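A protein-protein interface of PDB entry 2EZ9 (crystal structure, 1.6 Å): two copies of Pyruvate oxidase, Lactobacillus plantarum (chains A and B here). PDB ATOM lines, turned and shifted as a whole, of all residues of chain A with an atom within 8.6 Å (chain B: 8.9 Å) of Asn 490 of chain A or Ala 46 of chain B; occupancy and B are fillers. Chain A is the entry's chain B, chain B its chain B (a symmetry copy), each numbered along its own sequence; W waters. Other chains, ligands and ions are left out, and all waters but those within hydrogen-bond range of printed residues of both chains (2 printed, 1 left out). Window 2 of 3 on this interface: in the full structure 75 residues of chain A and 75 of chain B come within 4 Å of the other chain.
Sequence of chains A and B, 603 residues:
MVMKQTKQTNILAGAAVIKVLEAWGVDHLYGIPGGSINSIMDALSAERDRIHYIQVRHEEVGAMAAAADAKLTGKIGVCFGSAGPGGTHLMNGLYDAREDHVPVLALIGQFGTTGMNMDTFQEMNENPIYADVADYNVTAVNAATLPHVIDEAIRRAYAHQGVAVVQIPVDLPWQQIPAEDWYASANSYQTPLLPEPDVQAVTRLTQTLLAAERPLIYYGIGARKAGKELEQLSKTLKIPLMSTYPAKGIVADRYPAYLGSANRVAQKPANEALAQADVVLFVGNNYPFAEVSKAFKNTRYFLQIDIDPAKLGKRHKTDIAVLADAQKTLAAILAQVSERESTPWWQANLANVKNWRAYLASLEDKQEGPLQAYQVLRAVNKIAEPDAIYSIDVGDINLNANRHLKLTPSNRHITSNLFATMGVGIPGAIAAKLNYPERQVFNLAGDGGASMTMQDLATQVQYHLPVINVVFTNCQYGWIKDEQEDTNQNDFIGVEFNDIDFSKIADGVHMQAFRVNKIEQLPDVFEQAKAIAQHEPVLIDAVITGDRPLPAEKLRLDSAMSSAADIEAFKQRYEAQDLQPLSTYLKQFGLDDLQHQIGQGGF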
ATOM      1  N   GLN A 484       1.438  14.545 -11.295  1.00  0.00           N
ATOM      2  CA  GLN A 484       2.203  14.900 -10.094  1.00  0.00           C
ATOM      3  C   GLN A 484       1.283  15.180  -8.919  1.00  0.00           C
ATOM      4  O   GLN A 484       1.588  14.799  -7.786  1.00  0.00           O
ATOM      5  CB  GLN A 484       3.110  16.106 -10.357  1.00  0.00           C
ATOM      6  CG  GLN A 484       4.226  15.804 -11.361  1.00  0.00           C
ATOM      7  CD  GLN A 484       5.321  16.852 -11.383  1.00  0.00           C
ATOM      8  OE1 GLN A 484       5.205  17.913 -10.769  1.00  0.00           O
ATOM      9  NE2 GLN A 484       6.405  16.553 -12.098  1.00  0.00           N
ATOM     10  N   GLU A 485       0.150  15.830  -9.191  1.00  0.00           N
ATOM     11  CA  GLU A 485      -0.815  16.122  -8.134  1.00  0.00           C
ATOM     12  C   GLU A 485      -1.276  14.826  -7.498  1.00  0.00           C
ATOM     13  O   GLU A 485      -1.446  14.755  -6.272  1.00  0.00           O
ATOM     14  CB  GLU A 485      -2.013  16.882  -8.679  1.00  0.00           C
ATOM     15  CG  GLU A 485      -3.058  17.227  -7.600  1.00  0.00           C
ATOM     16  CD  GLU A 485      -4.275  17.882  -8.201  1.00  0.00           C
ATOM     17  OE1 GLU A 485      -4.180  19.068  -8.595  1.00  0.00           O
ATOM     18  OE2 GLU A 485      -5.328  17.207  -8.271  1.00  0.00           O
ATOM     19  N   ASP A 486      -1.441  13.801  -8.339  1.00  0.00           N
ATOM     20  CA  ASP A 486      -1.944  12.497  -7.907  1.00  0.00           C
ATOM     21  C   ASP A 486      -0.918  11.649  -7.170  1.00  0.00           C
ATOM     22  O   ASP A 486      -1.278  10.960  -6.218  1.00  0.00           O
ATOM     23  CB  ASP A 486      -2.496  11.711  -9.102  1.00  0.00           C
ATOM     24  CG  ASP A 486      -3.778  12.335  -9.683  1.00  0.00           C
ATOM     25  OD1 ASP A 486      -4.430  13.155  -8.995  1.00  0.00           O
ATOM     26  OD2 ASP A 486      -4.134  11.989 -10.825  1.00  0.00           O
ATOM     27  N   THR A 487       0.349  11.701  -7.598  1.00  0.00           N
ATOM     28  CA  THR A 487       1.365  10.763  -7.107  1.00  0.00           C
ATOM     29  C   THR A 487       2.499  11.373  -6.279  1.00  0.00           C
ATOM     30  O   THR A 487       3.077  10.690  -5.441  1.00  0.00           O
ATOM     31  CB  THR A 487       2.051  10.014  -8.276  1.00  0.00           C
ATOM     32  OG1 THR A 487       2.718  10.957  -9.128  1.00  0.00           O
ATOM     33  CG2 THR A 487       1.038   9.244  -9.096  1.00  0.00           C
ATOM     34  N   ASN A 488       2.857  12.622  -6.551  1.00  0.00           N
ATOM     35  CA  ASN A 488       4.095  13.169  -5.973  1.00  0.00           C
ATOM     36  C   ASN A 488       3.911  13.731  -4.571  1.00  0.00           C
ATOM     37  O   ASN A 488       2.887  14.350  -4.260  1.00  0.00           O
ATOM     38  CB  ASN A 488       4.701  14.213  -6.905  1.00  0.00           C
ATOM     39  CG  ASN A 488       5.356  13.585  -8.133  1.00  0.00           C
ATOM     40  OD1 ASN A 488       4.915  12.538  -8.625  1.00  0.00           O
ATOM     41  ND2 ASN A 488       6.416  14.219  -8.623  1.00  0.00           N
ATOM     42  N   GLN A 489       4.906  13.502  -3.722  1.00  0.00           N
ATOM     43  CA  GLN A 489       4.842  13.989  -2.348  1.00  0.00           C
ATOM     44  C   GLN A 489       5.295  15.442  -2.250  1.00  0.00           C
ATOM     45  O   GLN A 489       4.731  16.221  -1.484  1.00  0.00           O
ATOM     46  CB  GLN A 489       5.639  13.068  -1.419  1.00  0.00           C
ATOM     47  CG  GLN A 489       5.015  11.669  -1.281  1.00  0.00           C
ATOM     48  CD  GLN A 489       3.480  11.684  -1.163  1.00  0.00           C
ATOM     49  OE1 GLN A 489       2.933  11.997  -0.106  1.00  0.00           O
ATOM     50  NE2 GLN A 489       2.788  11.337  -2.254  1.00  0.00           N
ATOM     51  N   ASN A 490       6.302  15.801  -3.039  1.00  0.00           N
ATOM     52  CA  ASN A 490       6.873  17.143  -3.011  1.00  0.00           C
ATOM     53  C   ASN A 490       6.232  18.085  -4.037  1.00  0.00           C
ATOM     54  O   ASN A 490       5.320  17.680  -4.765  1.00  0.00           O
ATOM     55  CB  ASN A 490       8.394  17.049  -3.146  1.00  0.00           C
ATOM     56  CG  ASN A 490       8.995  16.125  -2.095  1.00  0.00           C
ATOM     57  OD1 ASN A 490       8.766  16.318  -0.901  1.00  0.00           O
ATOM     58  ND2 ASN A 490       9.732  15.108  -2.526  1.00  0.00           N
ATOM     59  N   ASP A 491       6.689  19.334  -4.073  1.00  0.00           N
ATOM     60  CA  ASP A 491       6.066  20.366  -4.914  1.00  0.00           C
ATOM     61  C   ASP A 491       6.127  20.010  -6.396  1.00  0.00           C
ATOM     62  O   ASP A 491       7.013  19.256  -6.832  1.00  0.00           O
ATOM     63  CB  ASP A 491       6.746  21.724  -4.716  1.00  0.00           C
ATOM     64  CG  ASP A 491       6.562  22.290  -3.315  1.00  0.00           C
ATOM     65  OD1 ASP A 491       5.787  21.720  -2.520  1.00  0.00           O
ATOM     66  OD2 ASP A 491       7.213  23.315  -3.007  1.00  0.00           O
ATOM     67  N   PHE A 492       5.204  20.590  -7.164  1.00  0.00           N
ATOM     68  CA  PHE A 492       5.252  20.504  -8.619  1.00  0.00           C
ATOM     69  C   PHE A 492       6.628  20.886  -9.129  1.00  0.00           C
ATOM     70  O   PHE A 492       7.259  21.822  -8.628  1.00  0.00           O
ATOM     71  CB  PHE A 492       4.229  21.451  -9.259  1.00  0.00           C
ATOM     72  CG  PHE A 492       2.792  21.057  -9.030  1.00  0.00           C
ATOM     73  CD1 PHE A 492       2.315  19.813  -9.440  1.00  0.00           C
ATOM     74  CD2 PHE A 492       1.899  21.957  -8.457  1.00  0.00           C
ATOM     75  CE1 PHE A 492       0.979  19.459  -9.260  1.00  0.00           C
ATOM     76  CE2 PHE A 492       0.561  21.611  -8.270  1.00  0.00           C
ATOM     77  CZ  PHE A 492       0.099  20.357  -8.671  1.00  0.00           C
ATOM     78  N   ILE A 493       7.089  20.172 -10.148  1.00  0.00           N
ATOM     79  CA  ILE A 493       8.396  20.477 -10.739  1.00  0.00           C
ATOM     80  C   ILE A 493       8.400  20.172 -12.237  1.00  0.00           C
ATOM     81  O   ILE A 493       7.960  19.099 -12.670  1.00  0.00           O
ATOM     82  CB  ILE A 493       9.541  19.735  -9.990  1.00  0.00           C
ATOM     83  CG1 ILE A 493      10.913  20.105 -10.567  1.00  0.00           C
ATOM     84  CG2 ILE A 493       9.306  18.217  -9.949  1.00  0.00           C
ATOM     85  CD1 ILE A 493      12.100  19.673  -9.675  1.00  0.00           C
ATOM     86  N   LEU B  12      14.224   7.133   0.784  1.00  0.00           N
ATOM     87  CA  LEU B  12      13.659   6.796  -0.521  1.00  0.00           C
ATOM     88  C   LEU B  12      14.799   6.568  -1.502  1.00  0.00           C
ATOM     89  O   LEU B  12      15.758   7.337  -1.539  1.00  0.00           O
ATOM     90  CB  LEU B  12      12.736   7.910  -1.026  1.00  0.00           C
ATOM     91  CG  LEU B  12      11.399   8.081  -0.297  1.00  0.00           C
ATOM     92  CD1 LEU B  12      10.667   9.253  -0.906  1.00  0.00           C
ATOM     93  CD2 LEU B  12      10.558   6.819  -0.414  1.00  0.00           C
ATOM     94  N   GLY B  14      14.956   7.135  -4.605  1.00  0.00           N
ATOM     95  CA  GLY B  14      15.070   8.371  -5.402  1.00  0.00           C
ATOM     96  C   GLY B  14      15.913   9.438  -4.716  1.00  0.00           C
ATOM     97  O   GLY B  14      16.770  10.063  -5.348  1.00  0.00           O
ATOM     98  N   ALA B  15      15.666   9.655  -3.427  1.00  0.00           N
ATOM     99  CA  ALA B  15      16.474  10.583  -2.636  1.00  0.00           C
ATOM    100  C   ALA B  15      17.956  10.200  -2.606  1.00  0.00           C
ATOM    101  O   ALA B  15      18.820  11.066  -2.739  1.00  0.00           O
ATOM    102  CB  ALA B  15      15.919  10.707  -1.218  1.00  0.00           C
ATOM    103  N   ILE B  18      19.614  11.128  -5.935  1.00  0.00           N
ATOM    104  CA  ILE B  18      19.954  12.550  -6.049  1.00  0.00           C
ATOM    105  C   ILE B  18      21.194  12.874  -5.212  1.00  0.00           C
ATOM    106  O   ILE B  18      22.042  13.663  -5.643  1.00  0.00           O
ATOM    107  CB  ILE B  18      18.755  13.490  -5.719  1.00  0.00           C
ATOM    108  CG1 ILE B  18      17.529  13.130  -6.571  1.00  0.00           C
ATOM    109  CG2 ILE B  18      19.133  14.957  -5.956  1.00  0.00           C
ATOM    110  CD1 ILE B  18      17.809  12.882  -8.059  1.00  0.00           C
ATOM    111  N   LYS B  19      21.321  12.230  -4.047  1.00  0.00           N
ATOM    112  CA  LYS B  19      22.534  12.369  -3.221  1.00  0.00           C
ATOM    113  C   LYS B  19      23.796  11.818  -3.898  1.00  0.00           C
ATOM    114  O   LYS B  19      24.898  12.357  -3.711  1.00  0.00           O
ATOM    115  CB  LYS B  19      22.342  11.752  -1.826  1.00  0.00           C
ATOM    116  CG  LYS B  19      21.296  12.466  -0.963  1.00  0.00           C
ATOM    117  CD  LYS B  19      21.648  13.923  -0.751  1.00  0.00           C
ATOM    118  CE  LYS B  19      20.635  14.637   0.129  1.00  0.00           C
ATOM    119  NZ  LYS B  19      21.135  16.019   0.398  1.00  0.00           N
ATOM    120  N   GLU B  22      24.766  14.580  -6.226  1.00  0.00           N
ATOM    121  CA  GLU B  22      25.351  15.679  -5.463  1.00  0.00           C
ATOM    122  C   GLU B  22      26.777  15.356  -5.026  1.00  0.00           C
ATOM    123  O   GLU B  22      27.650  16.233  -5.049  1.00  0.00           O
ATOM    124  CB  GLU B  22      24.464  16.044  -4.266  1.00  0.00           C
ATOM    125  CG  GLU B  22      23.131  16.648  -4.697  1.00  0.00           C
ATOM    126  CD  GLU B  22      22.159  16.859  -3.550  1.00  0.00           C
ATOM    127  OE1 GLU B  22      22.543  16.687  -2.373  1.00  0.00           O
ATOM    128  OE2 GLU B  22      21.000  17.194  -3.836  1.00  0.00           O
ATOM    129  N   ASN B  38       8.282  10.518 -12.917  1.00  0.00           N
ATOM    130  CA  ASN B  38       7.826  11.430 -11.871  1.00  0.00           C
ATOM    131  C   ASN B  38       8.400  11.156 -10.483  1.00  0.00           C
ATOM    132  O   ASN B  38       8.367  12.042  -9.619  1.00  0.00           O
ATOM    133  CB  ASN B  38       6.289  11.508 -11.806  1.00  0.00           C
ATOM    134  CG  ASN B  38       5.730  12.652 -12.638  1.00  0.00           C
ATOM    135  OD1 ASN B  38       6.438  13.616 -12.947  1.00  0.00           O
ATOM    136  ND2 ASN B  38       4.441  12.564 -12.988  1.00  0.00           N
ATOM    137  N   SER B  39       8.904   9.949 -10.251  1.00  0.00           N
ATOM    138  CA  SER B  39       9.485   9.649  -8.939  1.00  0.00           C
ATOM    139  C   SER B  39      10.895  10.234  -8.799  1.00  0.00           C
ATOM    140  O   SER B  39      11.295  10.622  -7.699  1.00  0.00           O
ATOM    141  CB  SER B  39       9.418   8.157  -8.593  1.00  0.00           C
ATOM    142  OG  SER B  39      10.083   7.348  -9.546  1.00  0.00           O
ATOM    143  N   ILE B  40      11.642  10.303  -9.905  1.00  0.00           N
ATOM    144  CA  ILE B  40      12.910  11.035  -9.913  1.00  0.00           C
ATOM    145  C   ILE B  40      12.631  12.540  -9.796  1.00  0.00           C
ATOM    146  O   ILE B  40      13.328  13.251  -9.065  1.00  0.00           O
ATOM    147  CB  ILE B  40      13.753  10.718 -11.177  1.00  0.00           C
ATOM    148  CG1 ILE B  40      14.346   9.300 -11.093  1.00  0.00           C
ATOM    149  CG2 ILE B  40      14.848  11.781 -11.419  1.00  0.00           C
ATOM    150  CD1 ILE B  40      15.416   9.062  -9.972  1.00  0.00           C
ATOM    151  N   MET B  41      11.613  13.021 -10.510  1.00  0.00           N
ATOM    152  CA  MET B  41      11.185  14.416 -10.374  1.00  0.00           C
ATOM    153  C   MET B  41      10.873  14.730  -8.913  1.00  0.00           C
ATOM    154  O   MET B  41      11.261  15.780  -8.407  1.00  0.00           O
ATOM    155  CB  MET B  41       9.938  14.704 -11.211  1.00  0.00           C
ATOM    156  CG  MET B  41      10.093  14.509 -12.717  1.00  0.00           C
ATOM    157  SD  MET B  41      11.510  15.341 -13.462  1.00  0.00           S
ATOM    158  CE  MET B  41      11.236  17.047 -12.974  1.00  0.00           C
ATOM    159  N   ASP B  42      10.191  13.810  -8.235  1.00  0.00           N
ATOM    160  CA  ASP B  42       9.796  14.015  -6.834  1.00  0.00           C
ATOM    161  C   ASP B  42      11.032  14.211  -5.951  1.00  0.00           C
ATOM    162  O   ASP B  42      11.064  15.110  -5.094  1.00  0.00           O
ATOM    163  CB  ASP B  42       8.966  12.825  -6.347  1.00  0.00           C
ATOM    164  CG  ASP B  42       7.925  13.204  -5.305  1.00  0.00           C
ATOM    165  OD1 ASP B  42       7.670  14.416  -5.092  1.00  0.00           O
ATOM    166  OD2 ASP B  42       7.344  12.271  -4.710  1.00  0.00           O
ATOM    167  N   ALA B  43      12.063  13.397  -6.180  1.00  0.00           N
ATOM    168  CA  ALA B  43      13.314  13.520  -5.417  1.00  0.00           C
ATOM    169  C   ALA B  43      14.050  14.835  -5.729  1.00  0.00           C
ATOM    170  O   ALA B  43      14.591  15.480  -4.817  1.00  0.00           O
ATOM    171  CB  ALA B  43      14.212  12.310  -5.670  1.00  0.00           C
ATOM    172  N   LEU B  44      14.071  15.233  -7.006  1.00  0.00           N
ATOM    173  CA  LEU B  44      14.652  16.518  -7.403  1.00  0.00           C
ATOM    174  C   LEU B  44      13.953  17.680  -6.724  1.00  0.00           C
ATOM    175  O   LEU B  44      14.606  18.626  -6.295  1.00  0.00           O
ATOM    176  CB  LEU B  44      14.590  16.735  -8.919  1.00  0.00           C
ATOM    177  CG  LEU B  44      15.563  15.885  -9.740  1.00  0.00           C
ATOM    178  CD1 LEU B  44      15.209  15.947 -11.228  1.00  0.00           C
ATOM    179  CD2 LEU B  44      17.034  16.276  -9.508  1.00  0.00           C
ATOM    180  N   SER B  45      12.627  17.589  -6.622  1.00  0.00           N
ATOM    181  CA  SER B  45      11.815  18.653  -6.043  1.00  0.00           C
ATOM    182  C   SER B  45      12.201  18.965  -4.598  1.00  0.00           C
ATOM    183  O   SER B  45      12.118  20.116  -4.177  1.00  0.00           O
ATOM    184  CB  SER B  45      10.340  18.274  -6.117  1.00  0.00           C
ATOM    185  OG  SER B  45       9.520  19.371  -5.748  1.00  0.00           O
ATOM    186  N   ALA B  46      12.606  17.942  -3.846  1.00  0.00           N
ATOM    187  CA  ALA B  46      13.027  18.113  -2.444  1.00  0.00           C
ATOM    188  C   ALA B  46      14.462  18.648  -2.294  1.00  0.00           C
ATOM    189  O   ALA B  46      14.874  19.035  -1.191  1.00  0.00           O
ATOM    190  CB  ALA B  46      12.894  16.797  -1.710  1.00  0.00           C
ATOM    191  N   GLU B  47      15.214  18.659  -3.398  1.00  0.00           N
ATOM    192  CA  GLU B  47      16.646  18.991  -3.373  1.00  0.00           C
ATOM    193  C   GLU B  47      17.003  20.229  -4.214  1.00  0.00           C
ATOM    194  O   GLU B  47      18.106  20.318  -4.771  1.00  0.00           O
ATOM    195  CB  GLU B  47      17.468  17.785  -3.859  1.00  0.00           C
ATOM    196  CG  GLU B  47      17.569  16.631  -2.863  1.00  0.00           C
ATOM    197  CD  GLU B  47      18.397  16.968  -1.627  1.00  0.00           C
ATOM    198  OE1 GLU B  47      19.504  17.540  -1.768  1.00  0.00           O
ATOM    199  OE2 GLU B  47      17.931  16.669  -0.504  1.00  0.00           O
ATOM    200  N   ARG B  48      16.089  21.189  -4.297  1.00  0.00           N
ATOM    201  CA  ARG B  48      16.295  22.382  -5.131  1.00  0.00           C
ATOM    202  C   ARG B  48      17.435  23.295  -4.681  1.00  0.00           C
ATOM    203  O   ARG B  48      17.986  24.049  -5.497  1.00  0.00           O
ATOM    204  CB  ARG B  48      15.006  23.187  -5.243  1.00  0.00           C
ATOM    205  CG  ARG B  48      13.914  22.471  -6.018  1.00  0.00           C
ATOM    206  CD  ARG B  48      12.672  23.334  -6.053  1.00  0.00           C
ATOM    207  NE  ARG B  48      11.437  22.557  -6.139  1.00  0.00           N
ATOM    208  CZ  ARG B  48      10.629  22.521  -7.196  1.00  0.00           C
ATOM    209  NH1 ARG B  48      10.925  23.197  -8.303  1.00  0.00           N
ATOM    210  NH2 ARG B  48       9.528  21.789  -7.152  1.00  0.00           N
ATOM    211  N   ASP B  49      17.785  23.231  -3.396  1.00  0.00           N
ATOM    212  CA  ASP B  49      18.881  24.041  -2.862  1.00  0.00           C
ATOM    213  C   ASP B  49      20.239  23.542  -3.360  1.00  0.00           C
ATOM    214  O   ASP B  49      21.144  24.342  -3.612  1.00  0.00           O
ATOM    215  CB  ASP B  49      18.852  24.069  -1.327  1.00  0.00           C
ATOM    216  CG  ASP B  49      19.968  24.927  -0.734  1.00  0.00           C
ATOM    217  OD1 ASP B  49      20.204  26.041  -1.252  1.00  0.00           O
ATOM    218  OD2 ASP B  49      20.611  24.489   0.247  1.00  0.00           O
ATOM    219  N   ARG B  50      20.363  22.225  -3.532  1.00  0.00           N
ATOM    220  CA  ARG B  50      21.665  21.595  -3.794  1.00  0.00           C
ATOM    221  C   ARG B  50      21.906  21.152  -5.237  1.00  0.00           C
ATOM    222  O   ARG B  50      23.054  20.979  -5.642  1.00  0.00           O
ATOM    223  CB  ARG B  50      21.878  20.412  -2.844  1.00  0.00           C
ATOM    224  CG  ARG B  50      22.377  20.804  -1.454  1.00  0.00           C
ATOM    225  CD  ARG B  50      22.506  19.587  -0.550  1.00  0.00           C
ATOM    226  NE  ARG B  50      21.215  19.151  -0.023  1.00  0.00           N
ATOM    227  CZ  ARG B  50      20.893  19.133   1.268  1.00  0.00           C
ATOM    228  NH1 ARG B  50      21.774  19.511   2.188  1.00  0.00           N
ATOM    229  NH2 ARG B  50      19.689  18.720   1.646  1.00  0.00           N
ATOM    230  N   ILE B  51      20.836  20.974  -6.008  1.00  0.00           N
ATOM    231  CA  ILE B  51      20.961  20.580  -7.414  1.00  0.00           C
ATOM    232  C   ILE B  51      19.906  21.328  -8.233  1.00  0.00           C
ATOM    233  O   ILE B  51      18.764  21.472  -7.798  1.00  0.00           O
ATOM    234  CB  ILE B  51      20.915  19.026  -7.603  1.00  0.00           C
ATOM    235  CG1 ILE B  51      21.442  18.628  -8.992  1.00  0.00           C
ATOM    236  CG2 ILE B  51      19.518  18.461  -7.309  1.00  0.00           C
ATOM    237  CD1 ILE B  51      21.835  17.163  -9.124  1.00  0.00           C
ATOM    238  N   TRP B 174      10.473   5.403  -5.542  1.00  0.00           N
ATOM    239  CA  TRP B 174       9.542   5.652  -4.422  1.00  0.00           C
ATOM    240  C   TRP B 174       9.613   4.576  -3.335  1.00  0.00           C
ATOM    241  O   TRP B 174       8.899   4.652  -2.331  1.00  0.00           O
ATOM    242  CB  TRP B 174       8.100   5.783  -4.930  1.00  0.00           C
ATOM    243  CG  TRP B 174       7.727   7.164  -5.400  1.00  0.00           C
ATOM    244  CD1 TRP B 174       8.047   8.364  -4.805  1.00  0.00           C
ATOM    245  CD2 TRP B 174       6.926   7.484  -6.542  1.00  0.00           C
ATOM    246  NE1 TRP B 174       7.509   9.407  -5.530  1.00  0.00           N
ATOM    247  CE2 TRP B 174       6.818   8.894  -6.599  1.00  0.00           C
ATOM    248  CE3 TRP B 174       6.309   6.713  -7.544  1.00  0.00           C
ATOM    249  CZ2 TRP B 174       6.115   9.550  -7.614  1.00  0.00           C
ATOM    250  CZ3 TRP B 174       5.610   7.376  -8.557  1.00  0.00           C
ATOM    251  CH2 TRP B 174       5.514   8.774  -8.574  1.00  0.00           C
HETATM  252  O   HOH W   1       9.229  20.376  -2.910  1.00  0.00           O
HETATM  253  O   HOH W   2       2.886  10.362 -11.825  1.00  0.00           O
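Water W2 lies within hydrogen-bond range of the side-chain hydroxyl of Thr 487 of chain A (2.8 Å) and the side-chain amide nitrogen of Asn 38 of chain B (2.9 Å).
Water W1 bridges N of Asp 491 of chain A (3.0 Å) and OG of Ser 45 of chain B (3.0 Å).
Of chain B, only Asp 42, Ser 45 and Ala 46 come within 4 Å of Asn 490 of chain A.
Of chain A, only Asn 490 comes within 4 Å of Ala 46 of chain B.
Of the printed residues of chain A, Ser 45 of chain B touches Asn 490, Asp 491 and Ile 493.
Of the printed residues of chain A, Asp 42 of chain B touches Asn 488 (3.5 Å), Gln 489 (2.9 Å) and Asn 490 (2.8 Å).
Printed residues of chain A within 4 Å of Trp 174 of chain B: Thr 487 (3.6 Å) and Asn 488 (3.4 Å).
Printed residues of chain B within 4 Å of Asp 491 of chain A: Ser 45 (2.7 Å) and Arg 48 (3.6 Å).
Of the printed residues of chain B, Gln 484 of chain A touches Asn 38.
Of the printed residues of chain B, Gln 489 of chain A touches Asp 42.
Asp 49 of chain B touches none of the printed residues of chain A.
Lys 19 of chain B touches none of the printed residues of chain A.
The nearest printed residue of chain A that does not touch Ala 46 of chain B is Asp 491 of chain A (6.1 Å).
No position is printed for both chains.
The side-chain hydroxyl of Ser 45 of chain B sits at hydrogen-bond distance from the guanidinium group of Arg 48 of chain B, at 2.8 Å.
NE2 of Gln 489 of chain A sits at hydrogen-bond distance from O of Thr 487 of chain A (3.3 Å).
The side-chain amide oxygen (OD1) of Asn 488 of chain A lies within hydrogen-bond range of the side-chain hydroxyl (OG1) of Thr 487 of chain A (2.8 Å).
The side-chain amide oxygen (OE1) of Gln 484 of chain A lies within hydrogen-bond range of the backbone NH (N) of Ile 493 of chain A (3.0 Å).
OD2 of Asp 42 of chain B sits at hydrogen-bond distance from NE1 of Trp 174 of chain B (3.0 Å).
The side-chain amide nitrogen of Gln 484 of chain A is in hydrogen-bond range of the side-chain amide oxygen of Asn 38 of chain B, 3.1 Å away.
O of Phe 492 of chain A lies within hydrogen-bond range of NH2 of Arg 48 of chain B (2.7 Å).
N of Asn 490 of chain A is in hydrogen-bond range of OD1 of Asp 42 of chain B.
OD2 of Asp 42 of chain B lies within hydrogen-bond range of N of Gln 489 of chain A.
The side-chain hydroxyl (OG) of Ser 45 of chain B lies within hydrogen-bond range of the backbone carbonyl oxygen (O) of Asp 491 of chain A (2.7 Å).
The side-chain amide nitrogen of Asn 488 of chain A sits at hydrogen-bond distance from the backbone carbonyl oxygen of Asn 38 of chain B (3.1 Å).
Among the printed residues, merely in contact across the chains: Asn 488 of chain A with Trp 174 of chain B (3.4 Å), Ile 493 of chain A with Met 41 of chain B (3.5 Å), Asn 488 of chain A with Asp 42 of chain B (3.5 Å), Ile 493 of chain A with Arg 48 of chain B (3.5 Å), Asp 491 of chain A with Arg 48 of chain B (3.6 Å), Thr 487 of chain A with Trp 174 of chain B (3.6 Å), Asn 490 of chain A with Ser 45 of chain B (3.7 Å), Asn 490 of chain A with Ala 46 of chain B (3.7 Å), Ile 493 of chain A with Ser 45 of chain B (3.7 Å) and Ile 493 of chain A with Leu 44 of chain B (3.9 Å).
Hydrophobic or aromatic side chains of chain A that line the printed part of chain B: Ile 493.
Of the 21 printed residues of chain B, 8 touch a printed residue of chain A.
Among the printed residues, 16 pairs touch across the chains.
Among the printed residues, no Asp or Glu carboxylate lies within 4 Å of a Lys or Arg side-chain nitrogen of the other chain.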
